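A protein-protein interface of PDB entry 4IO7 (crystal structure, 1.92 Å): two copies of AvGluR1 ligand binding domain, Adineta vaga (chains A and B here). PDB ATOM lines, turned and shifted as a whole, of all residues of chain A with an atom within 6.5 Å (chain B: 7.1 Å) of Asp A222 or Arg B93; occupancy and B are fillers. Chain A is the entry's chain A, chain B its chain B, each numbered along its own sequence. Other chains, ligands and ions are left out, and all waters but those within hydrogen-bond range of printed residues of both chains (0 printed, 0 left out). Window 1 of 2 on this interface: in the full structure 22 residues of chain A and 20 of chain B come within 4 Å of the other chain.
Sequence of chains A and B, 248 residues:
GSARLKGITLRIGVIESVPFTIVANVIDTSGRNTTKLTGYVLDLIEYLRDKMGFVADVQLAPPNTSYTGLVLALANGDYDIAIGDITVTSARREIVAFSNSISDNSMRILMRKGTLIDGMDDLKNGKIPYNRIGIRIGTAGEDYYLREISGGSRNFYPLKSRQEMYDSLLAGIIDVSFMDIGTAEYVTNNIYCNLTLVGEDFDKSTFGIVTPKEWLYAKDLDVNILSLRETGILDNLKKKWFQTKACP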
ATOM      1  N   MET A  52     -21.758  22.178 -22.368  1.00  0.00           N
ATOM      2  CA  MET A  52     -22.078  21.208 -21.339  1.00  0.00           C
ATOM      3  C   MET A  52     -23.071  20.134 -21.776  1.00  0.00           C
ATOM      4  O   MET A  52     -23.100  19.059 -21.193  1.00  0.00           O
ATOM      5  CB  MET A  52     -22.635  21.919 -20.135  1.00  0.00           C
ATOM      6  CG  MET A  52     -21.626  22.868 -19.491  1.00  0.00           C
ATOM      7  SD  MET A  52     -22.321  23.806 -18.123  1.00  0.00           S
ATOM      8  CE  MET A  52     -22.285  22.603 -16.847  1.00  0.00           C
ATOM      9  N   PHE A  98     -24.400  29.556  -4.876  1.00  0.00           N
ATOM     10  CA  PHE A  98     -24.142  30.349  -6.066  1.00  0.00           C
ATOM     11  C   PHE A  98     -22.964  29.781  -6.815  1.00  0.00           C
ATOM     12  O   PHE A  98     -21.986  29.345  -6.218  1.00  0.00           O
ATOM     13  CB  PHE A  98     -23.819  31.793  -5.682  1.00  0.00           C
ATOM     14  CG  PHE A  98     -24.995  32.579  -5.195  1.00  0.00           C
ATOM     15  CD1 PHE A  98     -25.287  32.639  -3.834  1.00  0.00           C
ATOM     16  CD2 PHE A  98     -25.819  33.249  -6.082  1.00  0.00           C
ATOM     17  CE1 PHE A  98     -26.364  33.369  -3.362  1.00  0.00           C
ATOM     18  CE2 PHE A  98     -26.921  33.986  -5.604  1.00  0.00           C
ATOM     19  CZ  PHE A  98     -27.188  34.037  -4.254  1.00  0.00           C
ATOM     20  N   SER A  99     -23.016  29.879  -8.131  1.00  0.00           N
ATOM     21  CA  SER A  99     -21.908  29.475  -8.972  1.00  0.00           C
ATOM     22  C   SER A  99     -20.797  30.475  -8.800  1.00  0.00           C
ATOM     23  O   SER A  99     -20.937  31.532  -8.195  1.00  0.00           O
ATOM     24  CB  SER A  99     -22.336  29.466 -10.446  1.00  0.00           C
ATOM     25  OG  SER A  99     -22.386  30.802 -10.978  1.00  0.00           O
ATOM     26  N   ASN A 100     -19.665  30.153  -9.366  1.00  0.00           N
ATOM     27  CA  ASN A 100     -18.634  31.151  -9.542  1.00  0.00           C
ATOM     28  C   ASN A 100     -19.246  32.381 -10.210  1.00  0.00           C
ATOM     29  O   ASN A 100     -20.157  32.280 -11.030  1.00  0.00           O
ATOM     30  CB  ASN A 100     -17.421  30.584 -10.296  1.00  0.00           C
ATOM     31  CG  ASN A 100     -16.541  29.742  -9.391  1.00  0.00           C
ATOM     32  OD1 ASN A 100     -16.490  28.520  -9.508  1.00  0.00           O
ATOM     33  ND2 ASN A 100     -15.898  30.389  -8.434  1.00  0.00           N
ATOM     34  N   SER A 101     -18.734  33.541  -9.821  1.00  0.00           N
ATOM     35  CA  SER A 101     -19.220  34.827 -10.305  1.00  0.00           C
ATOM     36  C   SER A 101     -19.275  34.932 -11.828  1.00  0.00           C
ATOM     37  O   SER A 101     -18.340  34.556 -12.508  1.00  0.00           O
ATOM     38  CB  SER A 101     -18.303  35.930  -9.783  1.00  0.00           C
ATOM     39  OG  SER A 101     -18.409  37.095 -10.580  1.00  0.00           O
ATOM     40  N   TYR A 217     -24.159  18.983  -9.353  1.00  0.00           N
ATOM     41  CA  TYR A 217     -23.516  19.445 -10.585  1.00  0.00           C
ATOM     42  C   TYR A 217     -22.681  20.700 -10.401  1.00  0.00           C
ATOM     43  O   TYR A 217     -22.340  21.367 -11.386  1.00  0.00           O
ATOM     44  CB  TYR A 217     -24.563  19.723 -11.668  1.00  0.00           C
ATOM     45  CG  TYR A 217     -25.512  18.585 -11.979  1.00  0.00           C
ATOM     46  CD1 TYR A 217     -25.110  17.510 -12.758  1.00  0.00           C
ATOM     47  CD2 TYR A 217     -26.835  18.618 -11.531  1.00  0.00           C
ATOM     48  CE1 TYR A 217     -25.988  16.483 -13.061  1.00  0.00           C
ATOM     49  CE2 TYR A 217     -27.719  17.608 -11.823  1.00  0.00           C
ATOM     50  CZ  TYR A 217     -27.292  16.542 -12.594  1.00  0.00           C
ATOM     51  OH  TYR A 217     -28.169  15.538 -12.881  1.00  0.00           O
ATOM     52  N   ALA A 218     -22.341  21.039  -9.156  1.00  0.00           N
ATOM     53  CA  ALA A 218     -21.726  22.340  -8.889  1.00  0.00           C
ATOM     54  C   ALA A 218     -20.392  22.539  -9.610  1.00  0.00           C
ATOM     55  O   ALA A 218     -20.135  23.601 -10.188  1.00  0.00           O
ATOM     56  CB  ALA A 218     -21.566  22.590  -7.361  1.00  0.00           C
ATOM     57  N   LYS A 219     -19.546  21.518  -9.567  1.00  0.00           N
ATOM     58  CA  LYS A 219     -18.223  21.592 -10.207  1.00  0.00           C
ATOM     59  C   LYS A 219     -18.348  21.787 -11.725  1.00  0.00           C
ATOM     60  O   LYS A 219     -17.676  22.646 -12.312  1.00  0.00           O
ATOM     61  CB  LYS A 219     -17.376  20.363  -9.865  1.00  0.00           C
ATOM     62  CG  LYS A 219     -15.956  20.391 -10.481  1.00  0.00           C
ATOM     63  CD  LYS A 219     -15.320  19.009 -10.565  1.00  0.00           C
ATOM     64  CE  LYS A 219     -15.966  18.086 -11.613  1.00  0.00           C
ATOM     65  NZ  LYS A 219     -15.820  18.567 -13.025  1.00  0.00           N
ATOM     66  N   ASP A 220     -19.227  21.023 -12.353  1.00  0.00           N
ATOM     67  CA  ASP A 220     -19.394  21.072 -13.804  1.00  0.00           C
ATOM     68  C   ASP A 220     -19.794  22.485 -14.235  1.00  0.00           C
ATOM     69  O   ASP A 220     -19.247  23.036 -15.171  1.00  0.00           O
ATOM     70  CB  ASP A 220     -20.436  20.007 -14.263  1.00  0.00           C
ATOM     71  CG  ASP A 220     -20.489  19.797 -15.810  1.00  0.00           C
ATOM     72  OD1 ASP A 220     -19.480  19.989 -16.515  1.00  0.00           O
ATOM     73  OD2 ASP A 220     -21.568  19.392 -16.341  1.00  0.00           O
ATOM     74  N   LEU A 221     -20.724  23.106 -13.524  1.00  0.00           N
ATOM     75  CA  LEU A 221     -21.145  24.442 -13.907  1.00  0.00           C
ATOM     76  C   LEU A 221     -20.040  25.459 -13.656  1.00  0.00           C
ATOM     77  O   LEU A 221     -19.791  26.330 -14.485  1.00  0.00           O
ATOM     78  CB  LEU A 221     -22.399  24.851 -13.135  1.00  0.00           C
ATOM     79  CG  LEU A 221     -22.897  26.262 -13.460  1.00  0.00           C
ATOM     80  CD1 LEU A 221     -23.349  26.366 -14.899  1.00  0.00           C
ATOM     81  CD2 LEU A 221     -24.022  26.620 -12.479  1.00  0.00           C
ATOM     82  N   ASP A 222     -19.384  25.353 -12.507  1.00  0.00           N
ATOM     83  CA  ASP A 222     -18.310  26.287 -12.160  1.00  0.00           C
ATOM     84  C   ASP A 222     -17.122  26.209 -13.132  1.00  0.00           C
ATOM     85  O   ASP A 222     -16.602  27.237 -13.540  1.00  0.00           O
ATOM     86  CB  ASP A 222     -17.784  26.037 -10.723  1.00  0.00           C
ATOM     87  CG  ASP A 222     -18.678  26.655  -9.616  1.00  0.00           C
ATOM     88  OD1 ASP A 222     -19.668  27.359  -9.922  1.00  0.00           O
ATOM     89  OD2 ASP A 222     -18.343  26.401  -8.432  1.00  0.00           O
ATOM     90  N   VAL A 223     -16.709  25.005 -13.515  1.00  0.00           N
ATOM     91  CA  VAL A 223     -15.551  24.859 -14.390  1.00  0.00           C
ATOM     92  C   VAL A 223     -15.895  25.517 -15.718  1.00  0.00           C
ATOM     93  O   VAL A 223     -15.082  26.212 -16.339  1.00  0.00           O
ATOM     94  CB  VAL A 223     -15.177  23.372 -14.531  1.00  0.00           C
ATOM     95  CG1 VAL A 223     -14.276  23.107 -15.724  1.00  0.00           C
ATOM     96  CG2 VAL A 223     -14.548  22.869 -13.197  1.00  0.00           C
ATOM     97  N   ASN A 224     -17.141  25.362 -16.114  1.00  0.00           N
ATOM     98  CA  ASN A 224     -17.569  25.879 -17.399  1.00  0.00           C
ATOM     99  C   ASN A 224     -17.709  27.402 -17.403  1.00  0.00           C
ATOM    100  O   ASN A 224     -17.292  28.058 -18.363  1.00  0.00           O
ATOM    101  CB  ASN A 224     -18.816  25.131 -17.884  1.00  0.00           C
ATOM    102  CG  ASN A 224     -18.482  23.845 -18.589  1.00  0.00           C
ATOM    103  OD1 ASN A 224     -18.115  23.882 -19.758  1.00  0.00           O
ATOM    104  ND2 ASN A 224     -18.566  22.699 -17.894  1.00  0.00           N
ATOM    105  N   ILE A 225     -18.269  27.985 -16.342  1.00  0.00           N
ATOM    106  CA  ILE A 225     -18.259  29.434 -16.179  1.00  0.00           C
ATOM    107  C   ILE A 225     -16.864  30.018 -16.193  1.00  0.00           C
ATOM    108  O   ILE A 225     -16.618  31.026 -16.846  1.00  0.00           O
ATOM    109  CB  ILE A 225     -18.934  29.853 -14.856  1.00  0.00           C
ATOM    110  CG1 ILE A 225     -20.425  29.538 -14.944  1.00  0.00           C
ATOM    111  CG2 ILE A 225     -18.732  31.314 -14.581  1.00  0.00           C
ATOM    112  CD1 ILE A 225     -21.075  29.621 -13.610  1.00  0.00           C
ATOM    113  N   LEU A 226     -15.946  29.403 -15.453  1.00  0.00           N
ATOM    114  CA  LEU A 226     -14.573  29.912 -15.408  1.00  0.00           C
ATOM    115  C   LEU A 226     -13.936  29.797 -16.797  1.00  0.00           C
ATOM    116  O   LEU A 226     -13.204  30.674 -17.218  1.00  0.00           O
ATOM    117  CB  LEU A 226     -13.748  29.168 -14.328  1.00  0.00           C
ATOM    118  CG  LEU A 226     -14.233  29.500 -12.920  1.00  0.00           C
ATOM    119  CD1 LEU A 226     -13.773  28.463 -11.892  1.00  0.00           C
ATOM    120  CD2 LEU A 226     -13.727  30.921 -12.557  1.00  0.00           C
ATOM    121  N   SER A 227     -14.242  28.740 -17.527  1.00  0.00           N
ATOM    122  CA  SER A 227     -13.719  28.599 -18.871  1.00  0.00           C
ATOM    123  C   SER A 227     -14.211  29.747 -19.811  1.00  0.00           C
ATOM    124  O   SER A 227     -13.408  30.332 -20.563  1.00  0.00           O
ATOM    125  CB  SER A 227     -14.046  27.210 -19.431  1.00  0.00           C
ATOM    126  OG  SER A 227     -13.625  27.098 -20.778  1.00  0.00           O
ATOM    127  N   VAL B  71      -2.372  24.544  -4.101  1.00  0.00           N
ATOM    128  CA  VAL B  71      -3.651  23.934  -4.454  1.00  0.00           C
ATOM    129  C   VAL B  71      -3.574  22.407  -4.492  1.00  0.00           C
ATOM    130  O   VAL B  71      -4.435  21.735  -3.948  1.00  0.00           O
ATOM    131  CB  VAL B  71      -4.170  24.504  -5.786  1.00  0.00           C
ATOM    132  CG1 VAL B  71      -5.455  23.778  -6.260  1.00  0.00           C
ATOM    133  CG2 VAL B  71      -4.419  25.990  -5.629  1.00  0.00           C
ATOM    134  N   VAL B  88      -8.911  32.176  -8.806  1.00  0.00           N
ATOM    135  CA  VAL B  88      -9.837  31.107  -9.122  1.00  0.00           C
ATOM    136  C   VAL B  88      -9.718  30.787 -10.618  1.00  0.00           C
ATOM    137  O   VAL B  88      -9.931  31.677 -11.458  1.00  0.00           O
ATOM    138  CB  VAL B  88     -11.285  31.539  -8.780  1.00  0.00           C
ATOM    139  CG1 VAL B  88     -12.250  30.387  -9.070  1.00  0.00           C
ATOM    140  CG2 VAL B  88     -11.371  31.976  -7.297  1.00  0.00           C
ATOM    141  N   THR B  89      -9.359  29.541 -10.966  1.00  0.00           N
ATOM    142  CA  THR B  89      -9.224  29.164 -12.378  1.00  0.00           C
ATOM    143  C   THR B  89     -10.010  27.893 -12.647  1.00  0.00           C
ATOM    144  O   THR B  89     -10.280  27.103 -11.718  1.00  0.00           O
ATOM    145  CB  THR B  89      -7.739  28.908 -12.820  1.00  0.00           C
ATOM    146  OG1 THR B  89      -7.305  27.676 -12.241  1.00  0.00           O
ATOM    147  CG2 THR B  89      -6.825  30.062 -12.401  1.00  0.00           C
ATOM    148  N   SER B  90     -10.337  27.670 -13.907  1.00  0.00           N
ATOM    149  CA  SER B  90     -11.101  26.474 -14.296  1.00  0.00           C
ATOM    150  C   SER B  90     -10.344  25.174 -13.983  1.00  0.00           C
ATOM    151  O   SER B  90     -10.924  24.215 -13.469  1.00  0.00           O
ATOM    152  CB  SER B  90     -11.503  26.509 -15.765  1.00  0.00           C
ATOM    153  OG  SER B  90     -10.410  26.541 -16.653  1.00  0.00           O
ATOM    154  N   ALA B  91      -9.051  25.162 -14.250  1.00  0.00           N
ATOM    155  CA  ALA B  91      -8.243  23.977 -13.975  1.00  0.00           C
ATOM    156  C   ALA B  91      -8.171  23.676 -12.458  1.00  0.00           C
ATOM    157  O   ALA B  91      -8.215  22.505 -12.062  1.00  0.00           O
ATOM    158  CB  ALA B  91      -6.839  24.151 -14.564  1.00  0.00           C
ATOM    159  N   ARG B  92      -8.053  24.708 -11.619  1.00  0.00           N
ATOM    160  CA  ARG B  92      -8.033  24.486 -10.165  1.00  0.00           C
ATOM    161  C   ARG B  92      -9.395  24.005  -9.690  1.00  0.00           C
ATOM    162  O   ARG B  92      -9.492  23.088  -8.860  1.00  0.00           O
ATOM    163  CB  ARG B  92      -7.576  25.751  -9.398  1.00  0.00           C
ATOM    164  CG  ARG B  92      -6.098  26.108  -9.669  1.00  0.00           C
ATOM    165  CD  ARG B  92      -5.693  27.466  -9.164  1.00  0.00           C
ATOM    166  NE  ARG B  92      -4.319  27.775  -9.519  1.00  0.00           N
ATOM    167  CZ  ARG B  92      -3.707  28.918  -9.234  1.00  0.00           C
ATOM    168  NH1 ARG B  92      -4.346  29.888  -8.589  1.00  0.00           N
ATOM    169  NH2 ARG B  92      -2.437  29.089  -9.587  1.00  0.00           N
ATOM    170  N   ARG B  93     -10.451  24.621 -10.227  1.00  0.00           N
ATOM    171  CA  ARG B  93     -11.815  24.305  -9.801  1.00  0.00           C
ATOM    172  C   ARG B  93     -12.171  22.844 -10.096  1.00  0.00           C
ATOM    173  O   ARG B  93     -13.033  22.263  -9.435  1.00  0.00           O
ATOM    174  CB  ARG B  93     -12.828  25.268 -10.435  1.00  0.00           C
ATOM    175  CG  ARG B  93     -14.291  24.947 -10.050  1.00  0.00           C
ATOM    176  CD  ARG B  93     -14.583  25.340  -8.562  1.00  0.00           C
ATOM    177  NE  ARG B  93     -15.940  24.950  -8.123  1.00  0.00           N
ATOM    178  CZ  ARG B  93     -16.238  23.764  -7.603  1.00  0.00           C
ATOM    179  NH1 ARG B  93     -15.320  22.801  -7.534  1.00  0.00           N
ATOM    180  NH2 ARG B  93     -17.464  23.494  -7.196  1.00  0.00           N
ATOM    181  N   GLU B  94     -11.447  22.221 -11.035  1.00  0.00           N
ATOM    182  CA  GLU B  94     -11.665  20.817 -11.357  1.00  0.00           C
ATOM    183  C   GLU B  94     -11.270  19.955 -10.147  1.00  0.00           C
ATOM    184  O   GLU B  94     -11.821  18.888  -9.936  1.00  0.00           O
ATOM    185  CB  GLU B  94     -10.839  20.441 -12.621  1.00  0.00           C
ATOM    186  CG  GLU B  94     -11.016  19.075 -13.140  1.00  0.00           C
ATOM    187  CD  GLU B  94     -12.436  18.824 -13.644  1.00  0.00           C
ATOM    188  OE1 GLU B  94     -12.924  19.577 -14.522  1.00  0.00           O
ATOM    189  OE2 GLU B  94     -13.038  17.856 -13.152  1.00  0.00           O
ATOM    190  N   ILE B  95     -10.346  20.441  -9.319  1.00  0.00           N
ATOM    191  CA  ILE B  95      -9.785  19.612  -8.237  1.00  0.00           C
ATOM    192  C   ILE B  95     -10.017  20.109  -6.798  1.00  0.00           C
ATOM    193  O   ILE B  95      -9.872  19.339  -5.853  1.00  0.00           O
ATOM    194  CB  ILE B  95      -8.278  19.322  -8.487  1.00  0.00           C
ATOM    195  CG1 ILE B  95      -7.443  20.609  -8.414  1.00  0.00           C
ATOM    196  CG2 ILE B  95      -8.121  18.630  -9.838  1.00  0.00           C
ATOM    197  CD1 ILE B  95      -5.899  20.354  -8.269  1.00  0.00           C
ATOM    198  N   VAL B  96     -10.431  21.367  -6.637  1.00  0.00           N
ATOM    199  CA  VAL B  96     -10.763  21.942  -5.324  1.00  0.00           C
ATOM    200  C   VAL B  96     -11.936  22.876  -5.514  1.00  0.00           C
ATOM    201  O   VAL B  96     -12.236  23.266  -6.638  1.00  0.00           O
ATOM    202  CB  VAL B  96      -9.570  22.781  -4.748  1.00  0.00           C
ATOM    203  CG1 VAL B  96      -8.343  21.866  -4.464  1.00  0.00           C
ATOM    204  CG2 VAL B  96      -9.210  23.890  -5.724  1.00  0.00           C
ATOM    205  N   ALA B  97     -12.601  23.232  -4.425  1.00  0.00           N
ATOM    206  CA  ALA B  97     -13.651  24.245  -4.482  1.00  0.00           C
ATOM    207  C   ALA B  97     -13.100  25.584  -4.013  1.00  0.00           C
ATOM    208  O   ALA B  97     -12.011  25.651  -3.468  1.00  0.00           O
ATOM    209  CB  ALA B  97     -14.914  23.815  -3.672  1.00  0.00           C
ATOM    210  N   PHE B  98     -13.827  26.667  -4.272  1.00  0.00           N
ATOM    211  CA  PHE B  98     -13.418  27.967  -3.766  1.00  0.00           C
ATOM    212  C   PHE B  98     -14.566  28.605  -3.017  1.00  0.00           C
ATOM    213  O   PHE B  98     -15.706  28.412  -3.354  1.00  0.00           O
ATOM    214  CB  PHE B  98     -13.033  28.887  -4.915  1.00  0.00           C
ATOM    215  CG  PHE B  98     -11.723  28.554  -5.553  1.00  0.00           C
ATOM    216  CD1 PHE B  98     -11.673  27.653  -6.601  1.00  0.00           C
ATOM    217  CD2 PHE B  98     -10.544  29.187  -5.141  1.00  0.00           C
ATOM    218  CE1 PHE B  98     -10.457  27.327  -7.208  1.00  0.00           C
ATOM    219  CE2 PHE B  98      -9.336  28.895  -5.764  1.00  0.00           C
ATOM    220  CZ  PHE B  98      -9.301  27.973  -6.803  1.00  0.00           C
ATOM    221  N   THR B 211     -10.933  25.377  -0.737  1.00  0.00           N
ATOM    222  CA  THR B 211     -11.446  24.389   0.187  1.00  0.00           C
ATOM    223  C   THR B 211     -11.500  23.066  -0.588  1.00  0.00           C
ATOM    224  O   THR B 211     -11.409  23.046  -1.823  1.00  0.00           O
ATOM    225  CB  THR B 211     -12.895  24.716   0.642  1.00  0.00           C
ATOM    226  OG1 THR B 211     -13.819  24.370  -0.401  1.00  0.00           O
ATOM    227  CG2 THR B 211     -13.094  26.222   0.987  1.00  0.00           C
ATOM    228  N   PRO B 212     -11.659  21.956   0.126  1.00  0.00           N
ATOM    229  CA  PRO B 212     -11.918  20.697  -0.573  1.00  0.00           C
ATOM    230  C   PRO B 212     -13.214  20.764  -1.355  1.00  0.00           C
ATOM    231  O   PRO B 212     -14.104  21.536  -0.996  1.00  0.00           O
ATOM    232  CB  PRO B 212     -12.065  19.679   0.573  1.00  0.00           C
ATOM    233  CG  PRO B 212     -11.351  20.294   1.746  1.00  0.00           C
ATOM    234  CD  PRO B 212     -11.639  21.777   1.594  1.00  0.00           C
ATOM    235  N   LYS B 213     -13.324  19.954  -2.407  1.00  0.00           N
ATOM    236  CA  LYS B 213     -14.590  19.800  -3.098  1.00  0.00           C
ATOM    237  C   LYS B 213     -15.615  19.176  -2.168  1.00  0.00           C
ATOM    238  O   LYS B 213     -15.271  18.351  -1.295  1.00  0.00           O
ATOM    239  CB  LYS B 213     -14.426  18.975  -4.382  1.00  0.00           C
ATOM    240  CG  LYS B 213     -13.596  19.710  -5.415  1.00  0.00           C
ATOM    241  CD  LYS B 213     -13.632  19.059  -6.744  1.00  0.00           C
ATOM    242  CE  LYS B 213     -13.088  17.652  -6.704  1.00  0.00           C
ATOM    243  NZ  LYS B 213     -13.272  17.094  -8.065  1.00  0.00           N
ATOM    244  N   GLU B 214     -16.860  19.614  -2.333  1.00  0.00           N
ATOM    245  CA  GLU B 214     -17.983  19.064  -1.585  1.00  0.00           C
ATOM    246  C   GLU B 214     -17.741  19.153  -0.082  1.00  0.00           C
ATOM    247  O   GLU B 214     -17.994  18.211   0.656  1.00  0.00           O
ATOM    248  CB  GLU B 214     -18.250  17.618  -2.026  1.00  0.00           C
ATOM    249  CG  GLU B 214     -18.576  17.532  -3.508  1.00  0.00           C
ATOM    250  CD  GLU B 214     -18.645  16.112  -4.028  1.00  0.00           C
ATOM    251  OE1 GLU B 214     -18.985  15.200  -3.255  1.00  0.00           O
ATOM    252  OE2 GLU B 214     -18.354  15.912  -5.219  1.00  0.00           O
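The side-chain amino group (NZ) of Lys A219 is in salt-bridge range of the side-chain carboxylate (OE2) of Glu B94 (2.9 Å). The guanidinium group (NE) of Arg B93 is in salt-bridge range of the side-chain carboxylate (OD2) of Asp A222.
OD1 of Asp A222 is in hydrogen-bond range of N of Asn A100 (2.8 Å). The backbone carbonyl oxygen of Glu B94 is in hydrogen-bond range of the side-chain amino group of Lys B213, at 3.0 Å. The guanidinium group (NH1) of Arg B93 lies within hydrogen-bond range of the backbone carbonyl oxygen (O) of Val B96 (3.2 Å). The backbone NH (N) of Arg B92 is in hydrogen-bond range of the side-chain hydroxyl (OG1) of Thr B89 (3.1 Å).
Asn A100 touches Val B88. OD1 of Asn A100 touches CD of Arg B93, at 3.8 Å. Ala A218 touches Arg B93. Lys B213 touches Lys A219 (NZ to CD, 3.8 Å). O of Val A223 touches CB of Ser B90, at 3.6 Å. Arg B93 touches Val A223 (CG to CG2, 3.8 Å). Val B88 touches Leu A226 (CG1 to CD1, 3.7 Å). Thr B89 touches Leu A226 (O to CD1, 3.8 Å). Ser B90 touches Leu A226. Arg B93 touches Leu A226.
Of the printed residues of chain B, Asp A222 touches Arg B93. Of the printed residues of chain A, Arg B93 touches Asn A100, Ala A218, Lys A219, Asp A222, Val A223 and Leu A226. Of the printed residues of chain B, Ser A227 touches Ser B90. Of the printed residues of chain B, Lys A219 touches Arg B93 (3.6 Å), Glu B94 (2.9 Å) and Lys B213 (3.8 Å). Of the printed residues of chain A, Lys B213 touches Lys A219 (3.8 Å). Val B71 touches none of the printed residues of chain A. Leu A221 touches none of the printed residues of chain B. The nearest printed residue of chain B that does not touch Lys A219 is Ile B95 (5.3 Å).
Of the 16 printed residues of chain A, 7 touch a printed residue of chain B. Printed residues of chain A that touch a printed residue of chain B: Asn A100, Ala A218, Lys A219, Asp A222, Val A223, Leu A226 and Ser A227. Hydrophobic or aromatic side chains of chain B that line the printed part of chain A: Val B88. Among the printed residues, 15 pairs touch across the chains.
Position printed for both chains: 98.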
